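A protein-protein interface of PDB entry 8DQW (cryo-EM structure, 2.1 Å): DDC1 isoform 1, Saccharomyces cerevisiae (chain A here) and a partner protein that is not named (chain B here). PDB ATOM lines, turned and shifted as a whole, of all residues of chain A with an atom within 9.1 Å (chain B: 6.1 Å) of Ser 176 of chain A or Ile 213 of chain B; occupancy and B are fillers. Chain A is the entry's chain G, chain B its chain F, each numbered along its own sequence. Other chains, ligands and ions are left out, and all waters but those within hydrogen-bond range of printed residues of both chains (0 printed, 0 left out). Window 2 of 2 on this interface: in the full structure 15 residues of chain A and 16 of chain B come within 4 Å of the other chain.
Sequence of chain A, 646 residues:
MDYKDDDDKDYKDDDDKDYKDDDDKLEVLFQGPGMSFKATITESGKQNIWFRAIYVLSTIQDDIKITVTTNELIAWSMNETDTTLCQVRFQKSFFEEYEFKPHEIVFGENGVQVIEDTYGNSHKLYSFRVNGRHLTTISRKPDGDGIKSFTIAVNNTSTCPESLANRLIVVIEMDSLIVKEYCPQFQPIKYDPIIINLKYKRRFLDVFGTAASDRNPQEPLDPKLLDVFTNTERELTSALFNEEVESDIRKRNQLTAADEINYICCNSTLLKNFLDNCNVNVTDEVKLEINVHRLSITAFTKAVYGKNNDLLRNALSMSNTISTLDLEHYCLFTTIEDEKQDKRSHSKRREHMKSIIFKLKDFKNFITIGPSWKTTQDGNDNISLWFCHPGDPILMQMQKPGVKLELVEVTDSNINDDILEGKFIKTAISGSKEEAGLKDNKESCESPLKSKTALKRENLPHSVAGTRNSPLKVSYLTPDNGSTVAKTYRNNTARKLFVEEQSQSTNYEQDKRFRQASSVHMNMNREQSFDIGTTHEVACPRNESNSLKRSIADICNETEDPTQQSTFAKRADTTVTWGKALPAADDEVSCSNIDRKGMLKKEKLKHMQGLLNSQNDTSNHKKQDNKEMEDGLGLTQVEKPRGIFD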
ATOM      1  N   PRO A 142       1.785  24.004 -22.269  1.00  0.00           N
ATOM      2  CA  PRO A 142       2.266  22.754 -21.671  1.00  0.00           C
ATOM      3  C   PRO A 142       2.551  22.928 -20.187  1.00  0.00           C
ATOM      4  O   PRO A 142       3.004  23.983 -19.737  1.00  0.00           O
ATOM      5  CB  PRO A 142       3.545  22.448 -22.459  1.00  0.00           C
ATOM      6  CG  PRO A 142       3.374  23.164 -23.748  1.00  0.00           C
ATOM      7  CD  PRO A 142       2.612  24.411 -23.418  1.00  0.00           C
ATOM      8  N   GLY A 144       4.849  21.619 -18.273  1.00  0.00           N
ATOM      9  CA  GLY A 144       6.248  21.799 -17.939  1.00  0.00           C
ATOM     10  C   GLY A 144       6.943  22.886 -18.733  1.00  0.00           C
ATOM     11  O   GLY A 144       7.618  23.746 -18.157  1.00  0.00           O
ATOM     12  N   ASP A 145       6.786  22.864 -20.053  1.00  0.00           N
ATOM     13  CA  ASP A 145       7.514  23.766 -20.934  1.00  0.00           C
ATOM     14  C   ASP A 145       6.705  25.027 -21.209  1.00  0.00           C
ATOM     15  O   ASP A 145       5.488  24.970 -21.410  1.00  0.00           O
ATOM     16  CB  ASP A 145       7.850  23.069 -22.254  1.00  0.00           C
ATOM     17  CG  ASP A 145       9.084  23.645 -22.921  1.00  0.00           C
ATOM     18  OD1 ASP A 145       9.586  24.688 -22.454  1.00  0.00           O
ATOM     19  OD2 ASP A 145       9.555  23.051 -23.914  1.00  0.00           O
ATOM     20  N   GLY A 146       7.399  26.175 -21.215  1.00  0.00           N
ATOM     21  CA  GLY A 146       6.767  27.440 -21.523  1.00  0.00           C
ATOM     22  C   GLY A 146       6.824  27.776 -23.005  1.00  0.00           C
ATOM     23  O   GLY A 146       7.497  27.117 -23.794  1.00  0.00           O
ATOM     24  N   ILE A 147       6.103  28.834 -23.371  1.00  0.00           N
ATOM     25  CA  ILE A 147       5.969  29.269 -24.758  1.00  0.00           C
ATOM     26  C   ILE A 147       6.604  30.644 -24.900  1.00  0.00           C
ATOM     27  O   ILE A 147       6.298  31.559 -24.125  1.00  0.00           O
ATOM     28  CB  ILE A 147       4.495  29.297 -25.196  1.00  0.00           C
ATOM     29  CG1 ILE A 147       3.951  27.872 -25.317  1.00  0.00           C
ATOM     30  CG2 ILE A 147       4.344  30.046 -26.516  1.00  0.00           C
ATOM     31  CD1 ILE A 147       2.441  27.791 -25.336  1.00  0.00           C
ATOM     32  N   LYS A 148       7.486  30.789 -25.889  1.00  0.00           N
ATOM     33  CA  LYS A 148       8.134  32.061 -26.186  1.00  0.00           C
ATOM     34  C   LYS A 148       7.309  32.889 -27.166  1.00  0.00           C
ATOM     35  O   LYS A 148       7.081  34.081 -26.935  1.00  0.00           O
ATOM     36  CB  LYS A 148       9.540  31.802 -26.743  1.00  0.00           C
ATOM     37  CG  LYS A 148      10.252  33.022 -27.336  1.00  0.00           C
ATOM     38  CD  LYS A 148      11.275  32.620 -28.397  1.00  0.00           C
ATOM     39  CE  LYS A 148      12.689  32.559 -27.838  1.00  0.00           C
ATOM     40  NZ  LYS A 148      13.523  33.699 -28.312  1.00  0.00           N
ATOM     41  N   ILE A 172       4.484  27.324 -32.817  1.00  0.00           N
ATOM     42  CA  ILE A 172       4.728  27.563 -31.401  1.00  0.00           C
ATOM     43  C   ILE A 172       6.212  27.355 -31.140  1.00  0.00           C
ATOM     44  O   ILE A 172       6.736  26.254 -31.346  1.00  0.00           O
ATOM     45  CB  ILE A 172       3.884  26.640 -30.509  1.00  0.00           C
ATOM     46  CG1 ILE A 172       2.420  26.638 -30.963  1.00  0.00           C
ATOM     47  CG2 ILE A 172       3.987  27.071 -29.051  1.00  0.00           C
ATOM     48  CD1 ILE A 172       1.550  25.655 -30.215  1.00  0.00           C
ATOM     49  N   GLU A 173       6.884  28.404 -30.680  1.00  0.00           N
ATOM     50  CA  GLU A 173       8.273  28.320 -30.255  1.00  0.00           C
ATOM     51  C   GLU A 173       8.312  28.138 -28.745  1.00  0.00           C
ATOM     52  O   GLU A 173       7.614  28.844 -28.012  1.00  0.00           O
ATOM     53  CB  GLU A 173       9.050  29.574 -30.658  1.00  0.00           C
ATOM     54  CG  GLU A 173       9.114  29.807 -32.162  1.00  0.00           C
ATOM     55  CD  GLU A 173      10.532  29.957 -32.689  1.00  0.00           C
ATOM     56  OE1 GLU A 173      11.470  30.103 -31.878  1.00  0.00           O
ATOM     57  OE2 GLU A 173      10.707  29.928 -33.925  1.00  0.00           O
ATOM     58  N   MET A 174       9.113  27.186 -28.287  1.00  0.00           N
ATOM     59  CA  MET A 174       9.258  26.913 -26.867  1.00  0.00           C
ATOM     60  C   MET A 174      10.512  27.589 -26.324  1.00  0.00           C
ATOM     61  O   MET A 174      11.437  27.930 -27.065  1.00  0.00           O
ATOM     62  CB  MET A 174       9.320  25.405 -26.611  1.00  0.00           C
ATOM     63  CG  MET A 174       8.176  24.624 -27.240  1.00  0.00           C
ATOM     64  SD  MET A 174       6.558  25.306 -26.831  1.00  0.00           S
ATOM     65  CE  MET A 174       6.351  24.687 -25.166  1.00  0.00           C
ATOM     66  N   ASP A 175      10.523  27.792 -25.006  1.00  0.00           N
ATOM     67  CA  ASP A 175      11.690  28.380 -24.358  1.00  0.00           C
ATOM     68  C   ASP A 175      12.920  27.495 -24.494  1.00  0.00           C
ATOM     69  O   ASP A 175      14.045  27.995 -24.398  1.00  0.00           O
ATOM     70  CB  ASP A 175      11.395  28.637 -22.880  1.00  0.00           C
ATOM     71  CG  ASP A 175      10.696  29.965 -22.644  1.00  0.00           C
ATOM     72  OD1 ASP A 175      10.525  30.736 -23.612  1.00  0.00           O
ATOM     73  OD2 ASP A 175      10.320  30.239 -21.485  1.00  0.00           O
ATOM     74  N   SER A 176      12.731  26.195 -24.714  1.00  0.00           N
ATOM     75  CA  SER A 176      13.825  25.259 -24.923  1.00  0.00           C
ATOM     76  C   SER A 176      14.254  25.179 -26.384  1.00  0.00           C
ATOM     77  O   SER A 176      14.946  24.228 -26.765  1.00  0.00           O
ATOM     78  CB  SER A 176      13.426  23.869 -24.422  1.00  0.00           C
ATOM     79  OG  SER A 176      12.243  23.423 -25.060  1.00  0.00           O
ATOM     80  N   LEU A 177      13.857  26.152 -27.203  1.00  0.00           N
ATOM     81  CA  LEU A 177      14.150  26.219 -28.633  1.00  0.00           C
ATOM     82  C   LEU A 177      13.428  25.138 -29.428  1.00  0.00           C
ATOM     83  O   LEU A 177      13.689  24.985 -30.628  1.00  0.00           O
ATOM     84  CB  LEU A 177      15.658  26.135 -28.908  1.00  0.00           C
ATOM     85  CG  LEU A 177      16.539  27.331 -28.518  1.00  0.00           C
ATOM     86  CD1 LEU A 177      17.707  27.452 -29.490  1.00  0.00           C
ATOM     87  CD2 LEU A 177      15.766  28.644 -28.447  1.00  0.00           C
ATOM     88  N   ILE A 178      12.525  24.384 -28.800  1.00  0.00           N
ATOM     89  CA  ILE A 178      11.702  23.429 -29.531  1.00  0.00           C
ATOM     90  C   ILE A 178      10.641  24.186 -30.316  1.00  0.00           C
ATOM     91  O   ILE A 178      10.104  25.202 -29.852  1.00  0.00           O
ATOM     92  CB  ILE A 178      11.065  22.417 -28.562  1.00  0.00           C
ATOM     93  CG1 ILE A 178      12.159  21.585 -27.882  1.00  0.00           C
ATOM     94  CG2 ILE A 178      10.056  21.520 -29.298  1.00  0.00           C
ATOM     95  CD1 ILE A 178      11.689  20.261 -27.313  1.00  0.00           C
ATOM     96  N   VAL A 179      10.335  23.699 -31.516  1.00  0.00           N
ATOM     97  CA  VAL A 179       9.345  24.310 -32.396  1.00  0.00           C
ATOM     98  C   VAL A 179       8.285  23.268 -32.723  1.00  0.00           C
ATOM     99  O   VAL A 179       8.613  22.137 -33.097  1.00  0.00           O
ATOM    100  CB  VAL A 179       9.988  24.856 -33.684  1.00  0.00           C
ATOM    101  CG1 VAL A 179       8.927  25.468 -34.592  1.00  0.00           C
ATOM    102  CG2 VAL A 179      11.064  25.878 -33.352  1.00  0.00           C
ATOM    103  N   LYS A 180       7.018  23.650 -32.577  1.00  0.00           N
ATOM    104  CA  LYS A 180       5.884  22.807 -32.926  1.00  0.00           C
ATOM    105  C   LYS A 180       5.068  23.493 -34.012  1.00  0.00           C
ATOM    106  O   LYS A 180       4.888  24.714 -33.987  1.00  0.00           O
ATOM    107  CB  LYS A 180       4.999  22.524 -31.704  1.00  0.00           C
ATOM    108  CG  LYS A 180       5.755  22.485 -30.382  1.00  0.00           C
ATOM    109  CD  LYS A 180       5.048  21.625 -29.337  1.00  0.00           C
ATOM    110  CE  LYS A 180       4.336  22.470 -28.290  1.00  0.00           C
ATOM    111  NZ  LYS A 180       4.208  21.753 -26.991  1.00  0.00           N
ATOM    112  N   ILE B 157      21.498  11.442 -30.093  1.00  0.00           N
ATOM    113  CA  ILE B 157      21.508  11.583 -28.641  1.00  0.00           C
ATOM    114  C   ILE B 157      20.663  12.798 -28.281  1.00  0.00           C
ATOM    115  O   ILE B 157      20.865  13.883 -28.837  1.00  0.00           O
ATOM    116  CB  ILE B 157      22.940  11.723 -28.092  1.00  0.00           C
ATOM    117  CG1 ILE B 157      23.759  10.476 -28.435  1.00  0.00           C
ATOM    118  CG2 ILE B 157      22.914  11.954 -26.582  1.00  0.00           C
ATOM    119  CD1 ILE B 157      25.206  10.538 -27.989  1.00  0.00           C
ATOM    120  N   ILE B 158      19.718  12.614 -27.356  1.00  0.00           N
ATOM    121  CA  ILE B 158      18.750  13.646 -27.009  1.00  0.00           C
ATOM    122  C   ILE B 158      18.628  13.748 -25.494  1.00  0.00           C
ATOM    123  O   ILE B 158      18.797  12.765 -24.763  1.00  0.00           O
ATOM    124  CB  ILE B 158      17.366  13.367 -27.643  1.00  0.00           C
ATOM    125  CG1 ILE B 158      17.469  13.311 -29.169  1.00  0.00           C
ATOM    126  CG2 ILE B 158      16.362  14.438 -27.229  1.00  0.00           C
ATOM    127  CD1 ILE B 158      16.302  12.617 -29.834  1.00  0.00           C
ATOM    128  N   LYS B 159      18.338  14.961 -25.026  1.00  0.00           N
ATOM    129  CA  LYS B 159      18.079  15.188 -23.611  1.00  0.00           C
ATOM    130  C   LYS B 159      16.738  14.578 -23.216  1.00  0.00           C
ATOM    131  O   LYS B 159      15.768  14.620 -23.978  1.00  0.00           O
ATOM    132  CB  LYS B 159      18.092  16.687 -23.305  1.00  0.00           C
ATOM    133  CG  LYS B 159      17.281  17.093 -22.069  1.00  0.00           C
ATOM    134  CD  LYS B 159      17.429  18.573 -21.716  1.00  0.00           C
ATOM    135  CE  LYS B 159      18.879  19.020 -21.570  1.00  0.00           C
ATOM    136  NZ  LYS B 159      19.761  17.996 -20.936  1.00  0.00           N
ATOM    137  N   ALA B 162      13.454  17.102 -23.023  1.00  0.00           N
ATOM    138  CA  ALA B 162      12.866  17.533 -24.288  1.00  0.00           C
ATOM    139  C   ALA B 162      12.080  16.405 -24.944  1.00  0.00           C
ATOM    140  O   ALA B 162      10.960  16.611 -25.432  1.00  0.00           O
ATOM    141  CB  ALA B 162      13.963  18.034 -25.224  1.00  0.00           C
ATOM    142  N   LEU B 163      12.655  15.202 -24.970  1.00  0.00           N
ATOM    143  CA  LEU B 163      11.957  14.065 -25.560  1.00  0.00           C
ATOM    144  C   LEU B 163      10.686  13.746 -24.787  1.00  0.00           C
ATOM    145  O   LEU B 163       9.651  13.426 -25.383  1.00  0.00           O
ATOM    146  CB  LEU B 163      12.876  12.847 -25.600  1.00  0.00           C
ATOM    147  CG  LEU B 163      12.279  11.601 -26.257  1.00  0.00           C
ATOM    148  CD1 LEU B 163      12.034  11.834 -27.742  1.00  0.00           C
ATOM    149  CD2 LEU B 163      13.177  10.402 -26.034  1.00  0.00           C
ATOM    150  N   SER B 165       8.850  15.836 -23.067  1.00  0.00           N
ATOM    151  CA  SER B 165       7.870  16.867 -23.391  1.00  0.00           C
ATOM    152  C   SER B 165       7.256  16.631 -24.767  1.00  0.00           C
ATOM    153  O   SER B 165       6.047  16.810 -24.957  1.00  0.00           O
ATOM    154  CB  SER B 165       8.521  18.248 -23.327  1.00  0.00           C
ATOM    155  OG  SER B 165       9.748  18.265 -24.034  1.00  0.00           O
ATOM    156  N   LEU B 207      13.316  19.291 -33.058  1.00  0.00           N
ATOM    157  CA  LEU B 207      14.308  19.438 -31.997  1.00  0.00           C
ATOM    158  C   LEU B 207      15.382  20.430 -32.432  1.00  0.00           C
ATOM    159  O   LEU B 207      15.887  20.329 -33.557  1.00  0.00           O
ATOM    160  CB  LEU B 207      14.947  18.096 -31.669  1.00  0.00           C
ATOM    161  CG  LEU B 207      14.368  17.347 -30.465  1.00  0.00           C
ATOM    162  CD1 LEU B 207      14.517  18.150 -29.180  1.00  0.00           C
ATOM    163  CD2 LEU B 207      12.908  16.996 -30.711  1.00  0.00           C
ATOM    164  N   PRO B 208      15.757  21.395 -31.592  1.00  0.00           N
ATOM    165  CA  PRO B 208      16.729  22.405 -32.025  1.00  0.00           C
ATOM    166  C   PRO B 208      18.089  21.791 -32.315  1.00  0.00           C
ATOM    167  O   PRO B 208      18.500  20.808 -31.694  1.00  0.00           O
ATOM    168  CB  PRO B 208      16.790  23.371 -30.837  1.00  0.00           C
ATOM    169  CG  PRO B 208      16.409  22.542 -29.664  1.00  0.00           C
ATOM    170  CD  PRO B 208      15.401  21.551 -30.169  1.00  0.00           C
ATOM    171  N   ASN B 210      21.119  22.321 -31.498  1.00  0.00           N
ATOM    172  CA  ASN B 210      22.040  22.875 -30.519  1.00  0.00           C
ATOM    173  C   ASN B 210      22.564  21.754 -29.635  1.00  0.00           C
ATOM    174  O   ASN B 210      21.869  20.766 -29.382  1.00  0.00           O
ATOM    175  CB  ASN B 210      21.363  23.952 -29.656  1.00  0.00           C
ATOM    176  CG  ASN B 210      22.322  24.611 -28.683  1.00  0.00           C
ATOM    177  OD1 ASN B 210      22.045  24.704 -27.487  1.00  0.00           O
ATOM    178  ND2 ASN B 210      23.456  25.077 -29.193  1.00  0.00           N
ATOM    179  N   ARG B 211      23.799  21.916 -29.161  1.00  0.00           N
ATOM    180  CA  ARG B 211      24.416  20.900 -28.317  1.00  0.00           C
ATOM    181  C   ARG B 211      23.990  21.063 -26.864  1.00  0.00           C
ATOM    182  O   ARG B 211      24.825  21.013 -25.956  1.00  0.00           O
ATOM    183  CB  ARG B 211      25.941  20.966 -28.431  1.00  0.00           C
ATOM    184  CG  ARG B 211      26.476  20.645 -29.816  1.00  0.00           C
ATOM    185  CD  ARG B 211      27.995  20.643 -29.836  1.00  0.00           C
ATOM    186  NE  ARG B 211      28.525  20.332 -31.159  1.00  0.00           N
ATOM    187  CZ  ARG B 211      29.816  20.289 -31.460  1.00  0.00           C
ATOM    188  NH1 ARG B 211      30.748  20.543 -30.555  1.00  0.00           N
ATOM    189  NH2 ARG B 211      30.182  19.985 -32.702  1.00  0.00           N
ATOM    190  N   SER B 212      22.698  21.249 -26.636  1.00  0.00           N
ATOM    191  CA  SER B 212      22.121  21.250 -25.297  1.00  0.00           C
ATOM    192  C   SER B 212      20.980  20.256 -25.170  1.00  0.00           C
ATOM    193  O   SER B 212      20.836  19.625 -24.120  1.00  0.00           O
ATOM    194  CB  SER B 212      21.621  22.655 -24.924  1.00  0.00           C
ATOM    195  OG  SER B 212      20.889  23.239 -25.987  1.00  0.00           O
ATOM    196  N   ILE B 213      20.173  20.096 -26.215  1.00  0.00           N
ATOM    197  CA  ILE B 213      19.111  19.105 -26.245  1.00  0.00           C
ATOM    198  C   ILE B 213      19.421  17.986 -27.231  1.00  0.00           C
ATOM    199  O   ILE B 213      19.225  16.810 -26.919  1.00  0.00           O
ATOM    200  CB  ILE B 213      17.756  19.769 -26.577  1.00  0.00           C
ATOM    201  CG1 ILE B 213      17.381  20.773 -25.485  1.00  0.00           C
ATOM    202  CG2 ILE B 213      16.670  18.717 -26.707  1.00  0.00           C
ATOM    203  CD1 ILE B 213      16.176  21.621 -25.822  1.00  0.00           C
ATOM    204  N   LEU B 214      19.906  18.333 -28.422  1.00  0.00           N
ATOM    205  CA  LEU B 214      20.328  17.357 -29.426  1.00  0.00           C
ATOM    206  C   LEU B 214      21.852  17.305 -29.384  1.00  0.00           C
ATOM    207  O   LEU B 214      22.538  18.070 -30.062  1.00  0.00           O
ATOM    208  CB  LEU B 214      19.806  17.737 -30.808  1.00  0.00           C
ATOM    209  CG  LEU B 214      20.141  16.779 -31.954  1.00  0.00           C
ATOM    210  CD1 LEU B 214      19.607  15.379 -31.677  1.00  0.00           C
ATOM    211  CD2 LEU B 214      19.593  17.314 -33.267  1.00  0.00           C
ATOM    212  N   GLU B 215      22.382  16.390 -28.570  1.00  0.00           N
ATOM    213  CA  GLU B 215      23.827  16.324 -28.378  1.00  0.00           C
ATOM    214  C   GLU B 215      24.544  16.002 -29.683  1.00  0.00           C
ATOM    215  O   GLU B 215      25.559  16.628 -30.011  1.00  0.00           O
ATOM    216  CB  GLU B 215      24.165  15.287 -27.308  1.00  0.00           C
ATOM    217  CG  GLU B 215      23.746  15.692 -25.902  1.00  0.00           C
ATOM    218  CD  GLU B 215      24.928  15.950 -24.986  1.00  0.00           C
ATOM    219  OE1 GLU B 215      25.989  16.383 -25.484  1.00  0.00           O
ATOM    220  OE2 GLU B 215      24.795  15.720 -23.766  1.00  0.00           O
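The backbone carbonyl oxygen (O) of Ile 213 of chain B sits at hydrogen-bond distance from the backbone NH (N) of Lys 159 of chain B (2.8 Å).
The side-chain hydroxyl (OG) of Ser 165 of chain B lies within hydrogen-bond range of the backbone carbonyl oxygen (O) of Ala 162 of chain B.
The side-chain carboxylate (OD2) of Asp 145 of chain A is in hydrogen-bond range of the side-chain hydroxyl (OG) of Ser 176 of chain A.
Among the printed residues, merely in contact across the chains: Ser 176 of chain A with Pro 208 of chain B, Ser 176 of chain A with Ile 213 of chain B, Leu 177 of chain A with Pro 208 of chain B, Ile 178 of chain A with Ala 162 of chain B, Ile 178 of chain A with Leu 207 of chain B and Ile 178 of chain A with Pro 208 of chain B.
Ile 213 of chain B touches just one residue of chain A: Ser 176 (3.0 Å).
Of the printed residues of chain A, Pro 208 of chain B touches Ser 176 (3.7 Å), Leu 177 (3.5 Å) and Ile 178 (3.97 Å).
Printed residues of chain A within 4 Å of Ala 162 of chain B: Ile 178.
Printed residues of chain B within 4 Å of Ile 178 of chain A: Ala 162, Leu 207 and Pro 208.
Of the printed residues of chain B, Leu 177 of chain A touches Pro 208.
Printed residues of chain A within 4 Å of Leu 207 of chain B: Ile 178.
Asp 145 of chain A touches none of the printed residues of chain B.
Asp 175 of chain A touches none of the printed residues of chain B.
The nearest residue of chain A that does not touch Ile 213 of chain B is Ile 178 of chain A (4.5 Å).
Printed residues of chain A that touch a printed residue of chain B: Ser 176, Leu 177 and Ile 178.
Hydrophobic or aromatic side chains of chain A that line the printed part of chain B: Leu 177 and Ile 178.
Along chain A the printed residues that touch a printed residue of chain B span positions 176 to 178.
Of the 14 printed residues of chain B, 4 touch a printed residue of chain A.
Printed residues of chain B that touch a printed residue of chain A: Ala 162, Leu 207, Pro 208 and Ile 213.
Among the printed residues, no Asp or Glu carboxylate lies within 4 Å of a Lys or Arg side-chain nitrogen of the other chain.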
